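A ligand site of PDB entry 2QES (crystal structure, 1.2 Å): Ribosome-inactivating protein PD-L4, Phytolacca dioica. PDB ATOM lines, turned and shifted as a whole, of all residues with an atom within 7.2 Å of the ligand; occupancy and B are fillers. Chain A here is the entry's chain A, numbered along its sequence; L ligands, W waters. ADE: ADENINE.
Water W1 bridges OE2 of Glu 175 (2.7 Å) and N9 of the ligand (2.8 Å).
The backbone carbonyl oxygen (O) of Ser 120 sits close to a nitrogen (N7) of the ligand (2.7 Å). The side-chain hydroxyl (OG) of Ser 120 sits close to a nitrogen (N6) of the ligand (3.4 Å). A nitrogen (N1) of the ligand lies within hydrogen-bond range of the backbone NH (N) of Val 73 (2.8 Å). The backbone carbonyl oxygen (O) of Val 73 is in hydrogen-bond range of a nitrogen (N6) of the ligand (3.1 Å). The guanidinium group of Arg 178 is in hydrogen-bond range of a nitrogen (N3) of the ligand, at 3.0 Å.
OD2 of Asp 91 lies within hydrogen-bond range of N of Ser 120 (2.9 Å). The side-chain hydroxyl of Ser 174 sits at hydrogen-bond distance from the guanidinium group of Arg 178, at 2.9 Å. NH1 of Arg 178 is in salt-bridge range of OE1 of Glu 175 (3.0 Å). The backbone carbonyl oxygen (O) of Asn 70 lies within hydrogen-bond range of the guanidinium group (NH2) of Arg 178. The backbone NH (N) of Tyr 72 lies close to the side-chain amide oxygen (OD1) of Asn 70. The backbone NH (N) of Glu 175 lies within hydrogen-bond range of the backbone carbonyl oxygen (O) of Ile 170, at 3.0 Å. The backbone carbonyl oxygen (O) of Leu 71 is in hydrogen-bond range of the side-chain hydroxyl (OG) of Ser 174 (2.8 Å). OH of Tyr 122 is in hydrogen-bond range of OE2 of Glu 175, at 2.6 Å.
O of Leu 71 touches C2 of the ligand, at 3.6 Å. Tyr 72 touches the ligand (CA to N1, 3.3 Å). Tyr 122 touches the ligand (CE2 to N9, 3.7 Å). CG2 of Ile 170 touches N3 of the ligand (3.5 Å). Ser 174 touches the ligand (OG to C2, 3.6 Å). Hydrophobic or aromatic side chains within 4 Å of the ligand: Tyr 72, Val 73, Tyr 122 and Ile 170. Eight residues have an atom within 4 Å of the ligand: Leu 71, Tyr 72, Val 73, Ser 120, Tyr 122, Ile 170, Ser 174 and Arg 178.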
ATOM      1  N   MET A  65      -9.758  -6.075  -7.959  1.00  0.00           N
ATOM      2  CA  MET A  65      -9.151  -7.060  -8.868  1.00  0.00           C
ATOM      3  C   MET A  65      -7.719  -7.305  -8.387  1.00  0.00           C
ATOM      4  O   MET A  65      -6.928  -6.369  -8.316  1.00  0.00           O
ATOM      5  CB  MET A  65      -9.179  -6.620 -10.294  1.00  0.00           C
ATOM      6  CG  MET A  65      -8.584  -7.628 -11.218  1.00  0.00           C
ATOM      7  SD  MET A  65      -9.060  -7.236 -12.890  1.00  0.00           S
ATOM      8  CE  MET A  65      -7.970  -8.285 -13.848  1.00  0.00           C
ATOM      9  N   LEU A  66      -7.397  -8.527  -8.099  1.00  0.00           N
ATOM     10  CA  LEU A  66      -6.096  -8.944  -7.605  1.00  0.00           C
ATOM     11  C   LEU A  66      -5.388  -9.800  -8.632  1.00  0.00           C
ATOM     12  O   LEU A  66      -5.950 -10.710  -9.257  1.00  0.00           O
ATOM     13  CB  LEU A  66      -6.184  -9.742  -6.321  1.00  0.00           C
ATOM     14  CG  LEU A  66      -6.503  -8.979  -5.038  1.00  0.00           C
ATOM     15  CD1 LEU A  66      -7.766  -8.191  -4.996  1.00  0.00           C
ATOM     16  CD2 LEU A  66      -6.527  -9.965  -3.845  1.00  0.00           C
ATOM     17  N   ASN A  70       1.193 -12.088  -7.429  1.00  0.00           N
ATOM     18  CA  ASN A  70       1.736 -11.336  -6.261  1.00  0.00           C
ATOM     19  C   ASN A  70       0.680 -10.746  -5.350  1.00  0.00           C
ATOM     20  O   ASN A  70       1.089 -10.041  -4.429  1.00  0.00           O
ATOM     21  CB  ASN A  70       2.659 -10.262  -6.778  1.00  0.00           C
ATOM     22  CG  ASN A  70       2.023  -9.233  -7.675  1.00  0.00           C
ATOM     23  OD1 ASN A  70       0.825  -9.176  -7.902  1.00  0.00           O
ATOM     24  ND2 ASN A  70       2.911  -8.368  -8.162  1.00  0.00           N
ATOM     25  N   LEU A  71      -0.568 -11.021  -5.580  1.00  0.00           N
ATOM     26  CA  LEU A  71      -1.740 -10.546  -4.778  1.00  0.00           C
ATOM     27  C   LEU A  71      -1.884  -9.040  -4.755  1.00  0.00           C
ATOM     28  O   LEU A  71      -2.572  -8.508  -3.901  1.00  0.00           O
ATOM     29  CB  LEU A  71      -1.736 -11.134  -3.363  1.00  0.00           C
ATOM     30  CG  LEU A  71      -2.522 -12.367  -3.009  1.00  0.00           C
ATOM     31  CD1 LEU A  71      -2.991 -12.211  -1.472  1.00  0.00           C
ATOM     32  CD2 LEU A  71      -3.618 -12.877  -3.832  1.00  0.00           C
ATOM     33  N   TYR A  72      -1.282  -8.363  -5.725  1.00  0.00           N
ATOM     34  CA  TYR A  72      -1.492  -6.897  -5.787  1.00  0.00           C
ATOM     35  C   TYR A  72      -2.880  -6.527  -6.285  1.00  0.00           C
ATOM     36  O   TYR A  72      -3.396  -7.161  -7.246  1.00  0.00           O
ATOM     37  CB  TYR A  72      -0.451  -6.248  -6.746  1.00  0.00           C
ATOM     38  CG  TYR A  72       0.749  -5.742  -6.004  1.00  0.00           C
ATOM     39  CD1 TYR A  72       1.074  -4.397  -6.030  1.00  0.00           C
ATOM     40  CD2 TYR A  72       1.558  -6.599  -5.261  1.00  0.00           C
ATOM     41  CE1 TYR A  72       2.158  -3.901  -5.370  1.00  0.00           C
ATOM     42  CE2 TYR A  72       2.659  -6.116  -4.576  1.00  0.00           C
ATOM     43  CZ  TYR A  72       2.981  -4.777  -4.623  1.00  0.00           C
ATOM     44  OH  TYR A  72       4.038  -4.248  -3.978  1.00  0.00           O
ATOM     45  N   VAL A  73      -3.486  -5.549  -5.669  1.00  0.00           N
ATOM     46  CA  VAL A  73      -4.712  -4.903  -6.144  1.00  0.00           C
ATOM     47  C   VAL A  73      -4.349  -4.047  -7.365  1.00  0.00           C
ATOM     48  O   VAL A  73      -3.513  -3.156  -7.277  1.00  0.00           O
ATOM     49  CB  VAL A  73      -5.346  -4.064  -5.046  1.00  0.00           C
ATOM     50  CG1 VAL A  73      -6.573  -3.350  -5.604  1.00  0.00           C
ATOM     51  CG2 VAL A  73      -5.781  -5.008  -3.884  1.00  0.00           C
ATOM     52  N   MET A  74      -4.962  -4.311  -8.489  1.00  0.00           N
ATOM     53  CA  MET A  74      -4.720  -3.676  -9.750  1.00  0.00           C
ATOM     54  C   MET A  74      -5.701  -2.529 -10.044  1.00  0.00           C
ATOM     55  O   MET A  74      -5.419  -1.654 -10.863  1.00  0.00           O
ATOM     56  CB  MET A  74      -4.825  -4.662 -10.914  1.00  0.00           C
ATOM     57  CG  MET A  74      -3.909  -5.891 -10.752  1.00  0.00           C
ATOM     58  SD  MET A  74      -4.206  -7.189 -11.954  1.00  0.00           S
ATOM     59  CE  MET A  74      -3.592  -6.463 -13.482  1.00  0.00           C
ATOM     60  N   GLY A  75      -6.853  -2.537  -9.388  1.00  0.00           N
ATOM     61  CA  GLY A  75      -7.941  -1.605  -9.614  1.00  0.00           C
ATOM     62  C   GLY A  75      -9.181  -2.131  -8.932  1.00  0.00           C
ATOM     63  O   GLY A  75      -9.163  -3.175  -8.251  1.00  0.00           O
ATOM     64  N   PHE A  89      -5.279   1.503 -11.463  1.00  0.00           N
ATOM     65  CA  PHE A  89      -4.038   2.124 -11.114  1.00  0.00           C
ATOM     66  C   PHE A  89      -3.243   2.502 -12.355  1.00  0.00           C
ATOM     67  O   PHE A  89      -3.298   1.847 -13.385  1.00  0.00           O
ATOM     68  CB  PHE A  89      -3.216   1.211 -10.169  1.00  0.00           C
ATOM     69  CG  PHE A  89      -3.573   1.275  -8.746  1.00  0.00           C
ATOM     70  CD1 PHE A  89      -3.427   2.413  -7.971  1.00  0.00           C
ATOM     71  CD2 PHE A  89      -4.047   0.127  -8.093  1.00  0.00           C
ATOM     72  CE1 PHE A  89      -3.708   2.444  -6.622  1.00  0.00           C
ATOM     73  CE2 PHE A  89      -4.337   0.130  -6.768  1.00  0.00           C
ATOM     74  CZ  PHE A  89      -4.161   1.283  -6.039  1.00  0.00           C
ATOM     75  N   ASP A  91      -0.119   2.332 -13.012  1.00  0.00           N
ATOM     76  CA  ASP A  91       1.113   1.558 -13.096  1.00  0.00           C
ATOM     77  C   ASP A  91       0.880   0.164 -13.713  1.00  0.00           C
ATOM     78  O   ASP A  91       1.806  -0.637 -13.650  1.00  0.00           O
ATOM     79  CB  ASP A  91       1.822   1.456 -11.764  1.00  0.00           C
ATOM     80  CG  ASP A  91       0.959   0.853 -10.661  1.00  0.00           C
ATOM     81  OD1 ASP A  91      -0.152   0.379 -10.927  1.00  0.00           O
ATOM     82  OD2 ASP A  91       1.477   0.839  -9.489  1.00  0.00           O
ATOM     83  N   ASN A 119       0.053   5.709  -8.751  1.00  0.00           N
ATOM     84  CA  ASN A 119       0.502   4.342  -8.709  1.00  0.00           C
ATOM     85  C   ASN A 119       0.088   3.699  -7.336  1.00  0.00           C
ATOM     86  O   ASN A 119      -0.448   4.329  -6.472  1.00  0.00           O
ATOM     87  CB  ASN A 119       1.967   4.166  -9.075  1.00  0.00           C
ATOM     88  CG  ASN A 119       2.930   4.634  -8.037  1.00  0.00           C
ATOM     89  OD1 ASN A 119       2.772   4.492  -6.813  1.00  0.00           O
ATOM     90  ND2 ASN A 119       4.033   5.211  -8.520  1.00  0.00           N
ATOM     91  N   SER A 120       0.367   2.386  -7.275  1.00  0.00           N
ATOM     92  CA  SER A 120      -0.172   1.661  -6.103  1.00  0.00           C
ATOM     93  C   SER A 120       0.866   1.377  -5.034  1.00  0.00           C
ATOM     94  O   SER A 120       0.608   0.600  -4.105  1.00  0.00           O
ATOM     95  CB  SER A 120      -0.815   0.345  -6.439  1.00  0.00           C
ATOM     96  OG  SER A 120       0.212  -0.575  -6.930  1.00  0.00           O
ATOM     97  N   GLN A 121       1.974   2.038  -5.097  1.00  0.00           N
ATOM     98  CA  GLN A 121       2.981   1.874  -4.045  1.00  0.00           C
ATOM     99  C   GLN A 121       2.483   2.444  -2.742  1.00  0.00           C
ATOM    100  O   GLN A 121       1.804   3.483  -2.720  1.00  0.00           O
ATOM    101  CB  GLN A 121       4.307   2.525  -4.468  1.00  0.00           C
ATOM    102  CG  GLN A 121       4.976   1.852  -5.585  1.00  0.00           C
ATOM    103  CD  GLN A 121       6.077   2.634  -6.275  1.00  0.00           C
ATOM    104  OE1 GLN A 121       6.954   3.208  -5.621  1.00  0.00           O
ATOM    105  NE2 GLN A 121       6.053   2.671  -7.611  1.00  0.00           N
ATOM    106  N   TYR A 122       2.809   1.829  -1.607  1.00  0.00           N
ATOM    107  CA  TYR A 122       2.422   2.451  -0.318  1.00  0.00           C
ATOM    108  C   TYR A 122       2.940   3.833  -0.167  1.00  0.00           C
ATOM    109  O   TYR A 122       2.231   4.677   0.414  1.00  0.00           O
ATOM    110  CB  TYR A 122       2.952   1.607   0.834  1.00  0.00           C
ATOM    111  CG  TYR A 122       2.193   0.373   1.161  1.00  0.00           C
ATOM    112  CD1 TYR A 122       0.807   0.360   1.253  1.00  0.00           C
ATOM    113  CD2 TYR A 122       2.848  -0.837   1.438  1.00  0.00           C
ATOM    114  CE1 TYR A 122       0.063  -0.761   1.584  1.00  0.00           C
ATOM    115  CE2 TYR A 122       2.131  -1.985   1.769  1.00  0.00           C
ATOM    116  CZ  TYR A 122       0.760  -1.947   1.826  1.00  0.00           C
ATOM    117  OH  TYR A 122       0.012  -3.019   2.153  1.00  0.00           O
ATOM    118  N   SER A 123       4.173   4.157  -0.646  1.00  0.00           N
ATOM    119  CA  SER A 123       4.657   5.531  -0.503  1.00  0.00           C
ATOM    120  C   SER A 123       3.652   6.521  -1.148  1.00  0.00           C
ATOM    121  O   SER A 123       3.368   7.563  -0.552  1.00  0.00           O
ATOM    122  CB  SER A 123       6.073   5.642  -1.089  1.00  0.00           C
ATOM    123  OG  SER A 123       6.000   5.163  -2.470  1.00  0.00           O
ATOM    124  N   LEU A 125       0.343   5.969  -1.922  1.00  0.00           N
ATOM    125  CA  LEU A 125      -0.942   5.955  -1.225  1.00  0.00           C
ATOM    126  C   LEU A 125      -0.901   6.777   0.054  1.00  0.00           C
ATOM    127  O   LEU A 125      -1.824   7.513   0.360  1.00  0.00           O
ATOM    128  CB  LEU A 125      -1.315   4.493  -0.926  1.00  0.00           C
ATOM    129  CG  LEU A 125      -1.591   3.610  -2.145  1.00  0.00           C
ATOM    130  CD1 LEU A 125      -1.842   2.184  -1.717  1.00  0.00           C
ATOM    131  CD2 LEU A 125      -2.671   4.179  -3.050  1.00  0.00           C
ATOM    132  N   LEU A 166      -8.098   2.526  -0.170  1.00  0.00           N
ATOM    133  CA  LEU A 166      -7.161   1.575  -0.758  1.00  0.00           C
ATOM    134  C   LEU A 166      -6.181   1.076   0.289  1.00  0.00           C
ATOM    135  O   LEU A 166      -5.876  -0.108   0.348  1.00  0.00           O
ATOM    136  CB  LEU A 166      -6.463   2.209  -1.934  1.00  0.00           C
ATOM    137  CG  LEU A 166      -7.349   2.413  -3.157  1.00  0.00           C
ATOM    138  CD1 LEU A 166      -6.690   3.339  -4.148  1.00  0.00           C
ATOM    139  CD2 LEU A 166      -7.723   1.083  -3.821  1.00  0.00           C
ATOM    140  N   ILE A 170      -6.313  -2.852   0.895  1.00  0.00           N
ATOM    141  CA  ILE A 170      -5.115  -3.575   0.557  1.00  0.00           C
ATOM    142  C   ILE A 170      -4.604  -4.368   1.758  1.00  0.00           C
ATOM    143  O   ILE A 170      -4.238  -5.554   1.637  1.00  0.00           O
ATOM    144  CB  ILE A 170      -4.015  -2.705  -0.051  1.00  0.00           C
ATOM    145  CG1 ILE A 170      -4.400  -2.243  -1.445  1.00  0.00           C
ATOM    146  CG2 ILE A 170      -2.664  -3.394  -0.010  1.00  0.00           C
ATOM    147  CD1 ILE A 170      -3.622  -1.053  -1.968  1.00  0.00           C
ATOM    148  N   GLN A 171      -4.535  -3.741   2.938  1.00  0.00           N
ATOM    149  CA  GLN A 171      -3.998  -4.415   4.107  1.00  0.00           C
ATOM    150  C   GLN A 171      -4.976  -5.465   4.676  1.00  0.00           C
ATOM    151  O   GLN A 171      -4.473  -6.538   5.063  1.00  0.00           O
ATOM    152  CB  GLN A 171      -3.542  -3.396   5.112  1.00  0.00           C
ATOM    153  CG  GLN A 171      -2.394  -2.611   4.578  1.00  0.00           C
ATOM    154  CD  GLN A 171      -1.929  -1.595   5.587  1.00  0.00           C
ATOM    155  OE1 GLN A 171      -0.988  -1.838   6.375  1.00  0.00           O
ATOM    156  NE2 GLN A 171      -2.568  -0.412   5.569  1.00  0.00           N
ATOM    157  N   SER A 174      -5.318  -8.129   0.908  1.00  0.00           N
ATOM    158  CA  SER A 174      -4.110  -8.780   0.380  1.00  0.00           C
ATOM    159  C   SER A 174      -3.072  -9.034   1.468  1.00  0.00           C
ATOM    160  O   SER A 174      -2.511 -10.132   1.533  1.00  0.00           O
ATOM    161  CB  SER A 174      -3.487  -7.917  -0.743  1.00  0.00           C
ATOM    162  OG  SER A 174      -2.238  -8.437  -1.103  1.00  0.00           O
ATOM    163  N   GLU A 175      -2.750  -8.080   2.343  1.00  0.00           N
ATOM    164  CA  GLU A 175      -1.723  -8.313   3.333  1.00  0.00           C
ATOM    165  C   GLU A 175      -2.175  -9.381   4.354  1.00  0.00           C
ATOM    166  O   GLU A 175      -1.358 -10.208   4.751  1.00  0.00           O
ATOM    167  CB  GLU A 175      -1.275  -7.057   4.075  1.00  0.00           C
ATOM    168  CG  GLU A 175      -0.663  -5.981   3.164  1.00  0.00           C
ATOM    169  CD  GLU A 175       0.696  -6.257   2.615  1.00  0.00           C
ATOM    170  OE1 GLU A 175       1.128  -7.410   2.594  1.00  0.00           O
ATOM    171  OE2 GLU A 175       1.326  -5.298   2.119  1.00  0.00           O
ATOM    172  N   ARG A 178      -1.725 -12.704   2.725  1.00  0.00           N
ATOM    173  CA  ARG A 178      -0.333 -13.091   2.699  1.00  0.00           C
ATOM    174  C   ARG A 178       0.185 -13.499   4.085  1.00  0.00           C
ATOM    175  O   ARG A 178       1.039 -14.381   4.180  1.00  0.00           O
ATOM    176  CB  ARG A 178       0.553 -11.924   2.249  1.00  0.00           C
ATOM    177  CG  ARG A 178       0.387 -11.513   0.792  1.00  0.00           C
ATOM    178  CD  ARG A 178       1.118 -10.241   0.564  1.00  0.00           C
ATOM    179  NE  ARG A 178       1.009  -9.738  -0.781  1.00  0.00           N
ATOM    180  CZ  ARG A 178       0.670  -8.480  -1.166  1.00  0.00           C
ATOM    181  NH1 ARG A 178       0.403  -7.529  -0.288  1.00  0.00           N
ATOM    182  NH2 ARG A 178       0.607  -8.187  -2.452  1.00  0.00           N
ATOM    183  N   GLU A 204       4.862  -6.744   5.852  1.00  0.00           N
ATOM    184  CA  GLU A 204       4.384  -6.239   4.570  1.00  0.00           C
ATOM    185  C   GLU A 204       5.531  -5.924   3.650  1.00  0.00           C
ATOM    186  O   GLU A 204       5.524  -6.226   2.468  1.00  0.00           O
ATOM    187  CB  GLU A 204       3.541  -4.992   4.815  1.00  0.00           C
ATOM    188  CG  GLU A 204       2.184  -5.233   5.468  1.00  0.00           C
ATOM    189  CD  GLU A 204       1.458  -3.966   5.755  1.00  0.00           C
ATOM    190  OE1 GLU A 204       2.005  -2.885   5.711  1.00  0.00           O
ATOM    191  OE2 GLU A 204       0.220  -4.057   6.070  1.00  0.00           O
ATOM    192  N   TRP A 207       7.825  -9.259   2.458  1.00  0.00           N
ATOM    193  CA  TRP A 207       7.206 -10.538   1.991  1.00  0.00           C
ATOM    194  C   TRP A 207       8.027 -11.248   0.946  1.00  0.00           C
ATOM    195  O   TRP A 207       8.169 -12.489   0.956  1.00  0.00           O
ATOM    196  CB  TRP A 207       5.845 -10.139   1.485  1.00  0.00           C
ATOM    197  CG  TRP A 207       5.006 -11.338   0.994  1.00  0.00           C
ATOM    198  CD1 TRP A 207       4.684 -12.469   1.666  1.00  0.00           C
ATOM    199  CD2 TRP A 207       4.391 -11.461  -0.314  1.00  0.00           C
ATOM    200  NE1 TRP A 207       3.875 -13.318   0.852  1.00  0.00           N
ATOM    201  CE2 TRP A 207       3.698 -12.663  -0.373  1.00  0.00           C
ATOM    202  CE3 TRP A 207       4.389 -10.573  -1.416  1.00  0.00           C
ATOM    203  CZ2 TRP A 207       2.981 -13.070  -1.491  1.00  0.00           C
ATOM    204  CZ3 TRP A 207       3.682 -10.970  -2.524  1.00  0.00           C
ATOM    205  CH2 TRP A 207       2.979 -12.182  -2.593  1.00  0.00           C
HETATM  206  N9  ADE L   1       1.326  -3.419  -1.495  1.00  0.00           N
HETATM  207  C8  ADE L   1       1.511  -2.209  -1.994  1.00  0.00           C
HETATM  208  N7  ADE L   1       0.607  -1.849  -2.904  1.00  0.00           N
HETATM  209  C5  ADE L   1      -0.231  -2.912  -3.041  1.00  0.00           C
HETATM  210  C6  ADE L   1      -1.331  -3.299  -3.861  1.00  0.00           C
HETATM  211  N6  ADE L   1      -1.699  -2.399  -4.833  1.00  0.00           N
HETATM  212  N1  ADE L   1      -1.873  -4.343  -3.669  1.00  0.00           N
HETATM  213  C2  ADE L   1      -1.408  -5.327  -2.713  1.00  0.00           C
HETATM  214  N3  ADE L   1      -0.351  -5.097  -1.965  1.00  0.00           N
HETATM  215  C4  ADE L   1       0.231  -3.896  -2.121  1.00  0.00           C
HETATM  216  O   HOH W   1       3.094  -4.853   0.105  1.00  0.00           O
